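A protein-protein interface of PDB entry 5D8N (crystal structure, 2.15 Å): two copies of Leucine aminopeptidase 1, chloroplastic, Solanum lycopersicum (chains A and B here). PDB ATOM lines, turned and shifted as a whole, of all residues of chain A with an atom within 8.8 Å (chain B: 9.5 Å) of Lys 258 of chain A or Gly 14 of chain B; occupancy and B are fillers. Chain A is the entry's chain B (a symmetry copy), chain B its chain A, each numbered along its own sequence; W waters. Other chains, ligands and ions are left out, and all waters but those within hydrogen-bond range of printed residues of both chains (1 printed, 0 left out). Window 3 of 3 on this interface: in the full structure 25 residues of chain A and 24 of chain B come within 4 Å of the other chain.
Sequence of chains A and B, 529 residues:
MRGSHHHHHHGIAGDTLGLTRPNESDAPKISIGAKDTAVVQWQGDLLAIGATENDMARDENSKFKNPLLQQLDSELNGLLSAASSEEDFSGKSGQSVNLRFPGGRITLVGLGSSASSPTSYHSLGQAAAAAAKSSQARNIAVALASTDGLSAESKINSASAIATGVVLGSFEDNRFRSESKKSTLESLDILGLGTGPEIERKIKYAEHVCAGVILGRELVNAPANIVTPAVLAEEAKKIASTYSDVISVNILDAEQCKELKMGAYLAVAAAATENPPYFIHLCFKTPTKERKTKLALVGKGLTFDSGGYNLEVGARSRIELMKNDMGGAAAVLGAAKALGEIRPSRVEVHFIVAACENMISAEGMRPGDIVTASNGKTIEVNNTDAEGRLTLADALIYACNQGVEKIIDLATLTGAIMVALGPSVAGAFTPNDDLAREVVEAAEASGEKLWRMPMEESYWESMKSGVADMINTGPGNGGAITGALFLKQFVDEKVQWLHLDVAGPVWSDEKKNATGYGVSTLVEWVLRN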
ATOM      1  N   LEU A 252      20.549 -27.496  -3.119  1.00  0.00           N
ATOM      2  CA  LEU A 252      19.117 -27.439  -2.845  1.00  0.00           C
ATOM      3  C   LEU A 252      18.366 -28.381  -3.751  1.00  0.00           C
ATOM      4  O   LEU A 252      18.534 -28.327  -4.978  1.00  0.00           O
ATOM      5  CB  LEU A 252      18.587 -26.020  -3.018  1.00  0.00           C
ATOM      6  CG  LEU A 252      19.367 -24.876  -2.359  1.00  0.00           C
ATOM      7  CD1 LEU A 252      18.555 -23.606  -2.480  1.00  0.00           C
ATOM      8  CD2 LEU A 252      19.524 -25.141  -0.882  1.00  0.00           C
ATOM      9  N   ASP A 253      17.461 -29.176  -3.183  1.00  0.00           N
ATOM     10  CA  ASP A 253      16.603 -30.021  -4.012  1.00  0.00           C
ATOM     11  C   ASP A 253      15.320 -29.311  -4.435  1.00  0.00           C
ATOM     12  O   ASP A 253      15.113 -28.125  -4.158  1.00  0.00           O
ATOM     13  CB  ASP A 253      16.333 -31.380  -3.338  1.00  0.00           C
ATOM     14  CG  ASP A 253      15.491 -31.265  -2.063  1.00  0.00           C
ATOM     15  OD1 ASP A 253      14.779 -30.248  -1.872  1.00  0.00           O
ATOM     16  OD2 ASP A 253      15.461 -32.271  -1.325  1.00  0.00           O
ATOM     17  N   ALA A 254      14.501 -29.980  -5.233  1.00  0.00           N
ATOM     18  CA  ALA A 254      13.323 -29.332  -5.827  1.00  0.00           C
ATOM     19  C   ALA A 254      12.399 -28.713  -4.783  1.00  0.00           C
ATOM     20  O   ALA A 254      11.840 -27.645  -5.008  1.00  0.00           O
ATOM     21  CB  ALA A 254      12.536 -30.332  -6.655  1.00  0.00           C
ATOM     22  N   GLU A 255      12.230 -29.392  -3.652  1.00  0.00           N
ATOM     23  CA  GLU A 255      11.307 -28.967  -2.600  1.00  0.00           C
ATOM     24  C   GLU A 255      11.833 -27.698  -1.957  1.00  0.00           C
ATOM     25  O   GLU A 255      11.081 -26.782  -1.676  1.00  0.00           O
ATOM     26  CB  GLU A 255      11.128 -30.059  -1.527  1.00  0.00           C
ATOM     27  CG  GLU A 255      10.085 -31.122  -1.860  1.00  0.00           C
ATOM     28  CD  GLU A 255       8.727 -30.565  -2.297  1.00  0.00           C
ATOM     29  OE1 GLU A 255       7.978 -30.018  -1.444  1.00  0.00           O
ATOM     30  OE2 GLU A 255       8.403 -30.689  -3.508  1.00  0.00           O
ATOM     31  N   GLN A 256      13.134 -27.638  -1.708  1.00  0.00           N
ATOM     32  CA  GLN A 256      13.732 -26.422  -1.199  1.00  0.00           C
ATOM     33  C   GLN A 256      13.617 -25.252  -2.186  1.00  0.00           C
ATOM     34  O   GLN A 256      13.396 -24.100  -1.800  1.00  0.00           O
ATOM     35  CB  GLN A 256      15.199 -26.684  -0.862  1.00  0.00           C
ATOM     36  CG  GLN A 256      15.410 -27.653   0.289  1.00  0.00           C
ATOM     37  CD  GLN A 256      16.868 -28.049   0.440  1.00  0.00           C
ATOM     38  OE1 GLN A 256      17.398 -28.839  -0.330  1.00  0.00           O
ATOM     39  NE2 GLN A 256      17.537 -27.442   1.404  1.00  0.00           N
ATOM     40  N   CYS A 257      13.791 -25.512  -3.479  1.00  0.00           N
ATOM     41  CA  CYS A 257      13.638 -24.422  -4.461  1.00  0.00           C
ATOM     42  C   CYS A 257      12.176 -23.963  -4.539  1.00  0.00           C
ATOM     43  O   CYS A 257      11.865 -22.785  -4.793  1.00  0.00           O
ATOM     44  CB  CYS A 257      14.142 -24.877  -5.846  1.00  0.00           C
ATOM     45  SG  CYS A 257      15.933 -25.168  -5.912  1.00  0.00           S
ATOM     46  N   LYS A 258      11.265 -24.892  -4.260  1.00  0.00           N
ATOM     47  CA  LYS A 258       9.845 -24.536  -4.261  1.00  0.00           C
ATOM     48  C   LYS A 258       9.500 -23.610  -3.090  1.00  0.00           C
ATOM     49  O   LYS A 258       8.781 -22.643  -3.258  1.00  0.00           O
ATOM     50  CB  LYS A 258       8.988 -25.792  -4.166  1.00  0.00           C
ATOM     51  CG  LYS A 258       7.485 -25.567  -4.199  1.00  0.00           C
ATOM     52  CD  LYS A 258       6.831 -26.931  -4.390  1.00  0.00           C
ATOM     53  CE  LYS A 258       5.322 -26.815  -4.419  1.00  0.00           C
ATOM     54  NZ  LYS A 258       4.727 -28.168  -4.596  1.00  0.00           N
ATOM     55  N   GLU A 259      10.103 -23.862  -1.933  1.00  0.00           N
ATOM     56  CA  GLU A 259       9.964 -22.967  -0.787  1.00  0.00           C
ATOM     57  C   GLU A 259      10.565 -21.605  -1.077  1.00  0.00           C
ATOM     58  O   GLU A 259      10.152 -20.614  -0.506  1.00  0.00           O
ATOM     59  CB  GLU A 259      10.652 -23.561   0.459  1.00  0.00           C
ATOM     60  CG  GLU A 259       9.860 -24.668   1.132  1.00  0.00           C
ATOM     61  N   LEU A 260      11.580 -21.550  -1.928  1.00  0.00           N
ATOM     62  CA  LEU A 260      12.143 -20.277  -2.353  1.00  0.00           C
ATOM     63  C   LEU A 260      11.440 -19.700  -3.582  1.00  0.00           C
ATOM     64  O   LEU A 260      11.813 -18.643  -4.103  1.00  0.00           O
ATOM     65  CB  LEU A 260      13.626 -20.439  -2.627  1.00  0.00           C
ATOM     66  CG  LEU A 260      14.473 -20.672  -1.378  1.00  0.00           C
ATOM     67  CD1 LEU A 260      15.894 -21.020  -1.769  1.00  0.00           C
ATOM     68  CD2 LEU A 260      14.482 -19.428  -0.503  1.00  0.00           C
ATOM     69  N   LYS A 261      10.336 -20.320  -3.946  1.00  0.00           N
ATOM     70  CA  LYS A 261       9.423 -19.786  -4.956  1.00  0.00           C
ATOM     71  C   LYS A 261       9.995 -19.715  -6.377  1.00  0.00           C
ATOM     72  O   LYS A 261       9.597 -18.864  -7.169  1.00  0.00           O
ATOM     73  CB  LYS A 261       8.864 -18.417  -4.539  1.00  0.00           C
ATOM     74  CG  LYS A 261       8.173 -18.431  -3.183  1.00  0.00           C
ATOM     75  CD  LYS A 261       7.547 -17.071  -2.874  1.00  0.00           C
ATOM     76  CE  LYS A 261       8.632 -16.005  -2.717  1.00  0.00           C
ATOM     77  N   MET A 262      10.838 -20.671  -6.731  1.00  0.00           N
ATOM     78  CA  MET A 262      11.540 -20.631  -8.001  1.00  0.00           C
ATOM     79  C   MET A 262      10.679 -21.273  -9.069  1.00  0.00           C
ATOM     80  O   MET A 262      11.005 -22.333  -9.601  1.00  0.00           O
ATOM     81  CB  MET A 262      12.867 -21.374  -7.902  1.00  0.00           C
ATOM     82  CG  MET A 262      13.866 -20.780  -6.925  1.00  0.00           C
ATOM     83  SD  MET A 262      15.469 -21.576  -7.171  1.00  0.00           S
ATOM     84  CE  MET A 262      16.340 -20.926  -5.758  1.00  0.00           C
ATOM     85  N   GLY A 263       9.572 -20.629  -9.386  1.00  0.00           N
ATOM     86  CA  GLY A 263       8.624 -21.220 -10.305  1.00  0.00           C
ATOM     87  C   GLY A 263       9.122 -21.313 -11.744  1.00  0.00           C
ATOM     88  O   GLY A 263       8.658 -22.177 -12.490  1.00  0.00           O
ATOM     89  N   TYR A 265      12.337 -21.866 -12.819  1.00  0.00           N
ATOM     90  CA  TYR A 265      13.290 -22.975 -12.866  1.00  0.00           C
ATOM     91  C   TYR A 265      12.559 -24.312 -12.691  1.00  0.00           C
ATOM     92  O   TYR A 265      12.686 -25.200 -13.528  1.00  0.00           O
ATOM     93  CB  TYR A 265      14.328 -22.782 -11.762  1.00  0.00           C
ATOM     94  CG  TYR A 265      15.176 -23.978 -11.363  1.00  0.00           C
ATOM     95  CD1 TYR A 265      15.836 -24.748 -12.299  1.00  0.00           C
ATOM     96  CD2 TYR A 265      15.365 -24.304 -10.024  1.00  0.00           C
ATOM     97  CE1 TYR A 265      16.702 -25.759 -11.923  1.00  0.00           C
ATOM     98  CE2 TYR A 265      16.212 -25.322  -9.634  1.00  0.00           C
ATOM     99  CZ  TYR A 265      16.903 -26.036 -10.589  1.00  0.00           C
ATOM    100  OH  TYR A 265      17.773 -27.024 -10.196  1.00  0.00           O
ATOM    101  N   LEU A 266      11.620 -24.356 -11.754  1.00  0.00           N
ATOM    102  CA  LEU A 266      10.918 -25.587 -11.493  1.00  0.00           C
ATOM    103  C   LEU A 266       9.995 -25.955 -12.660  1.00  0.00           C
ATOM    104  O   LEU A 266       9.824 -27.144 -12.956  1.00  0.00           O
ATOM    105  CB  LEU A 266      10.180 -25.542 -10.149  1.00  0.00           C
ATOM    106  CG  LEU A 266      11.147 -25.499  -8.952  1.00  0.00           C
ATOM    107  CD1 LEU A 266      10.411 -25.251  -7.654  1.00  0.00           C
ATOM    108  CD2 LEU A 266      11.869 -26.837  -8.834  1.00  0.00           C
ATOM    109  N   PHE A 279      19.832 -27.477  -7.396  1.00  0.00           N
ATOM    110  CA  PHE A 279      20.309 -26.114  -7.465  1.00  0.00           C
ATOM    111  C   PHE A 279      21.625 -26.099  -6.673  1.00  0.00           C
ATOM    112  O   PHE A 279      21.664 -26.343  -5.462  1.00  0.00           O
ATOM    113  CB  PHE A 279      19.243 -25.186  -6.875  1.00  0.00           C
ATOM    114  CG  PHE A 279      19.517 -23.718  -7.054  1.00  0.00           C
ATOM    115  CD1 PHE A 279      20.458 -23.063  -6.261  1.00  0.00           C
ATOM    116  CD2 PHE A 279      18.883 -23.003  -8.058  1.00  0.00           C
ATOM    117  CE1 PHE A 279      20.665 -21.702  -6.382  1.00  0.00           C
ATOM    118  CE2 PHE A 279      19.057 -21.638  -8.162  1.00  0.00           C
ATOM    119  CZ  PHE A 279      19.994 -20.994  -7.371  1.00  0.00           C
ATOM    120  N   THR A 372       5.815 -18.223 -12.802  1.00  0.00           N
ATOM    121  CA  THR A 372       6.089 -17.092 -11.922  1.00  0.00           C
ATOM    122  C   THR A 372       7.457 -17.265 -11.276  1.00  0.00           C
ATOM    123  O   THR A 372       7.703 -18.212 -10.514  1.00  0.00           O
ATOM    124  CB  THR A 372       4.985 -16.989 -10.852  1.00  0.00           C
ATOM    125  OG1 THR A 372       3.699 -16.931 -11.485  1.00  0.00           O
ATOM    126  CG2 THR A 372       5.149 -15.751  -9.983  1.00  0.00           C
ATOM    127  N   SER A 374      10.815 -16.156  -8.870  1.00  0.00           N
ATOM    128  CA  SER A 374      10.891 -15.977  -7.430  1.00  0.00           C
ATOM    129  C   SER A 374      10.876 -14.514  -7.038  1.00  0.00           C
ATOM    130  O   SER A 374      10.817 -14.205  -5.861  1.00  0.00           O
ATOM    131  CB  SER A 374      12.115 -16.707  -6.849  1.00  0.00           C
ATOM    132  OG  SER A 374      13.294 -16.406  -7.566  1.00  0.00           O
ATOM    133  N   ASP A 394      15.648 -17.404 -12.026  1.00  0.00           N
ATOM    134  CA  ASP A 394      15.626 -17.746 -10.611  1.00  0.00           C
ATOM    135  C   ASP A 394      17.033 -17.830 -10.026  1.00  0.00           C
ATOM    136  O   ASP A 394      17.250 -17.484  -8.865  1.00  0.00           O
ATOM    137  CB  ASP A 394      14.858 -19.044 -10.389  1.00  0.00           C
ATOM    138  CG  ASP A 394      13.348 -18.819 -10.357  1.00  0.00           C
ATOM    139  OD1 ASP A 394      12.932 -17.769  -9.805  1.00  0.00           O
ATOM    140  OD2 ASP A 394      12.589 -19.699 -10.845  1.00  0.00           O
ATOM    141  N   ALA B  13      -0.305 -21.638  -4.715  1.00  0.00           N
ATOM    142  CA  ALA B  13      -0.074 -22.129  -6.104  1.00  0.00           C
ATOM    143  C   ALA B  13       0.843 -23.353  -6.092  1.00  0.00           C
ATOM    144  O   ALA B  13       1.361 -23.744  -7.137  1.00  0.00           O
ATOM    145  CB  ALA B  13       0.517 -21.022  -6.968  1.00  0.00           C
ATOM    146  N   GLY B  14       1.042 -23.938  -4.909  1.00  0.00           N
ATOM    147  CA  GLY B  14       1.909 -25.091  -4.706  1.00  0.00           C
ATOM    148  C   GLY B  14       1.762 -26.233  -5.696  1.00  0.00           C
ATOM    149  O   GLY B  14       2.766 -26.811  -6.079  1.00  0.00           O
ATOM    150  N   ASP B  15       0.546 -26.588  -6.111  1.00  0.00           N
ATOM    151  CA  ASP B  15       0.367 -27.647  -7.116  1.00  0.00           C
ATOM    152  C   ASP B  15       0.188 -27.160  -8.562  1.00  0.00           C
ATOM    153  O   ASP B  15       0.018 -27.969  -9.463  1.00  0.00           O
ATOM    154  CB  ASP B  15      -0.826 -28.530  -6.763  1.00  0.00           C
ATOM    155  CG  ASP B  15      -0.634 -29.270  -5.450  1.00  0.00           C
ATOM    156  OD1 ASP B  15       0.497 -29.738  -5.169  1.00  0.00           O
ATOM    157  OD2 ASP B  15      -1.635 -29.364  -4.702  1.00  0.00           O
ATOM    158  N   THR B  16       0.254 -25.856  -8.789  1.00  0.00           N
ATOM    159  CA  THR B  16       0.304 -25.324 -10.132  1.00  0.00           C
ATOM    160  C   THR B  16       1.727 -25.313 -10.700  1.00  0.00           C
ATOM    161  O   THR B  16       2.672 -24.826 -10.076  1.00  0.00           O
ATOM    162  CB  THR B  16      -0.289 -23.913 -10.104  1.00  0.00           C
ATOM    163  OG1 THR B  16      -1.649 -24.016  -9.670  1.00  0.00           O
ATOM    164  CG2 THR B  16      -0.264 -23.257 -11.472  1.00  0.00           C
ATOM    165  N   LEU B  17       1.883 -25.829 -11.910  1.00  0.00           N
ATOM    166  CA  LEU B  17       3.158 -25.725 -12.621  1.00  0.00           C
ATOM    167  C   LEU B  17       3.577 -24.271 -12.822  1.00  0.00           C
ATOM    168  O   LEU B  17       2.764 -23.424 -13.162  1.00  0.00           O
ATOM    169  CB  LEU B  17       3.086 -26.437 -13.974  1.00  0.00           C
ATOM    170  CG  LEU B  17       4.377 -26.410 -14.808  1.00  0.00           C
ATOM    171  CD1 LEU B  17       4.517 -27.690 -15.626  1.00  0.00           C
ATOM    172  CD2 LEU B  17       4.420 -25.202 -15.720  1.00  0.00           C
ATOM    173  N   GLY B  18       4.804 -23.948 -12.431  1.00  0.00           N
ATOM    174  CA  GLY B  18       5.283 -22.564 -12.446  1.00  0.00           C
ATOM    175  C   GLY B  18       4.879 -21.698 -11.268  1.00  0.00           C
ATOM    176  O   GLY B  18       5.200 -20.513 -11.228  1.00  0.00           O
ATOM    177  N   LEU B  19       4.134 -22.283 -10.340  1.00  0.00           N
ATOM    178  CA  LEU B  19       3.736 -21.637  -9.091  1.00  0.00           C
ATOM    179  C   LEU B  19       2.907 -20.379  -9.314  1.00  0.00           C
ATOM    180  O   LEU B  19       2.959 -19.452  -8.523  1.00  0.00           O
ATOM    181  CB  LEU B  19       4.974 -21.326  -8.235  1.00  0.00           C
ATOM    182  CG  LEU B  19       5.797 -22.557  -7.890  1.00  0.00           C
ATOM    183  CD1 LEU B  19       7.033 -22.169  -7.091  1.00  0.00           C
ATOM    184  CD2 LEU B  19       4.947 -23.565  -7.121  1.00  0.00           C
ATOM    185  N   THR B  20       2.159 -20.353 -10.409  1.00  0.00           N
ATOM    186  CA  THR B  20       1.426 -19.182 -10.801  1.00  0.00           C
ATOM    187  C   THR B  20       0.105 -19.118 -10.052  1.00  0.00           C
ATOM    188  O   THR B  20      -0.583 -20.122  -9.871  1.00  0.00           O
ATOM    189  CB  THR B  20       1.261 -19.139 -12.322  1.00  0.00           C
ATOM    190  OG1 THR B  20       2.563 -18.971 -12.898  1.00  0.00           O
ATOM    191  CG2 THR B  20       0.346 -17.992 -12.761  1.00  0.00           C
ATOM    192  N   ARG B  21      -0.184 -17.935  -9.536  1.00  0.00           N
ATOM    193  CA  ARG B  21      -1.406 -17.720  -8.769  1.00  0.00           C
ATOM    194  C   ARG B  21      -2.199 -16.588  -9.412  1.00  0.00           C
ATOM    195  O   ARG B  21      -1.745 -15.453  -9.500  1.00  0.00           O
ATOM    196  CB  ARG B  21      -1.056 -17.383  -7.321  1.00  0.00           C
ATOM    197  CG  ARG B  21      -2.275 -17.161  -6.439  1.00  0.00           C
ATOM    198  CD  ARG B  21      -1.872 -16.715  -5.038  1.00  0.00           C
ATOM    199  NE  ARG B  21      -3.007 -16.469  -4.151  1.00  0.00           N
ATOM    200  CZ  ARG B  21      -2.918 -16.426  -2.823  1.00  0.00           C
ATOM    201  NH1 ARG B  21      -1.750 -16.587  -2.218  1.00  0.00           N
ATOM    202  NH2 ARG B  21      -3.999 -16.232  -2.084  1.00  0.00           N
ATOM    203  N   PRO B  22      -3.352 -16.910  -9.979  1.00  0.00           N
ATOM    204  CA  PRO B  22      -4.155 -15.813 -10.545  1.00  0.00           C
ATOM    205  C   PRO B  22      -4.529 -14.759  -9.508  1.00  0.00           C
ATOM    206  O   PRO B  22      -4.809 -15.089  -8.355  1.00  0.00           O
ATOM    207  CB  PRO B  22      -5.425 -16.498 -11.039  1.00  0.00           C
ATOM    208  CG  PRO B  22      -5.150 -17.966 -10.957  1.00  0.00           C
ATOM    209  CD  PRO B  22      -4.051 -18.201  -9.965  1.00  0.00           C
ATOM    210  N   GLU B 274      -0.769 -36.527 -16.013  1.00  0.00           N
ATOM    211  CA  GLU B 274      -0.666 -35.647 -14.855  1.00  0.00           C
ATOM    212  C   GLU B 274      -1.946 -34.818 -14.691  1.00  0.00           C
ATOM    213  O   GLU B 274      -2.295 -34.429 -13.582  1.00  0.00           O
ATOM    214  CB  GLU B 274       0.536 -34.727 -15.001  1.00  0.00           C
ATOM    215  CG  GLU B 274       0.840 -33.891 -13.764  1.00  0.00           C
ATOM    216  CD  GLU B 274       1.293 -34.705 -12.549  1.00  0.00           C
ATOM    217  OE1 GLU B 274       1.406 -35.955 -12.613  1.00  0.00           O
ATOM    218  OE2 GLU B 274       1.511 -34.080 -11.487  1.00  0.00           O
HETATM  219  O   HOH W   1       1.588 -15.693 -10.214  1.00  0.00           O
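No position is printed for both chains.
The side-chain hydroxyl (OG1) of Thr 20 of chain B lies within hydrogen-bond range of the backbone carbonyl oxygen (O) of Gly 18 of chain B, 3.5 Å away.
The backbone NH of Ser 374 of chain A lies close to the backbone carbonyl oxygen of Lys 261 of chain A, at 3.4 Å.
The backbone NH (N) of Gly 263 of chain A sits close to the backbone carbonyl oxygen (O) of Thr 372 of chain A.
OD2 of Asp 394 of chain A is in hydrogen-bond range of N of Gly 263 of chain A, 3.5 Å away.
Of the 11 printed residues of chain B, 4 touch a printed residue of chain A.
Along chain B the printed residues that touch a printed residue of chain A span positions 14 to 20.
Among the printed residues, 7 pairs touch across the chains.
Water W1 bridges the side-chain hydroxyl (OG1) of Thr 372 of chain A (2.8 Å) and the backbone NH (N) of Arg 21 of chain B (2.9 Å).
Among the printed residues, pairs that only touch across the chains: Gly 263 of chain A with Gly 18 of chain B, Gly 263 of chain A with Leu 19 of chain B, Lys 261 of chain A with Leu 19 of chain B and Thr 372 of chain A with Leu 19 of chain B.
Of chain A, only Lys 258 (2.8 Å) comes within 4 Å of Gly 14 of chain B.
No residue of chain B comes within 4 Å of Cys 257 of chain A.
No residue of chain B comes within 4 Å of Glu 259 of chain A.
No residue of chain A comes within 4 Å of Ala 13 of chain B.
No residue of chain A comes within 4 Å of Asp 15 of chain B.
Of the printed residues of chain A, Gly 18 of chain B touches Gly 263 (3.4 Å) and Thr 372 (2.8 Å).
Of the printed residues of chain B, Thr 372 of chain A touches Gly 18 (2.8 Å), Leu 19 (3.9 Å) and Thr 20 (2.7 Å).
Printed residues of chain A within 4 Å of Thr 20 of chain B: Thr 372 (2.7 Å).
Of the printed residues of chain B, Lys 261 of chain A touches Leu 19.
Asp 253 of chain A touches none of the printed residues of chain B.
Asp 394 of chain A touches none of the printed residues of chain B.
The backbone carbonyl oxygen (O) of Gly 14 of chain B sits at hydrogen-bond distance from the side-chain amino group (NZ) of Lys 258 of chain A.
The backbone NH of Thr 372 of chain A is in hydrogen-bond range of the backbone carbonyl oxygen of Gly 18 of chain B (2.8 Å).
OG1 of Thr 372 of chain A is in hydrogen-bond range of OG1 of Thr 20 of chain B (2.7 Å).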
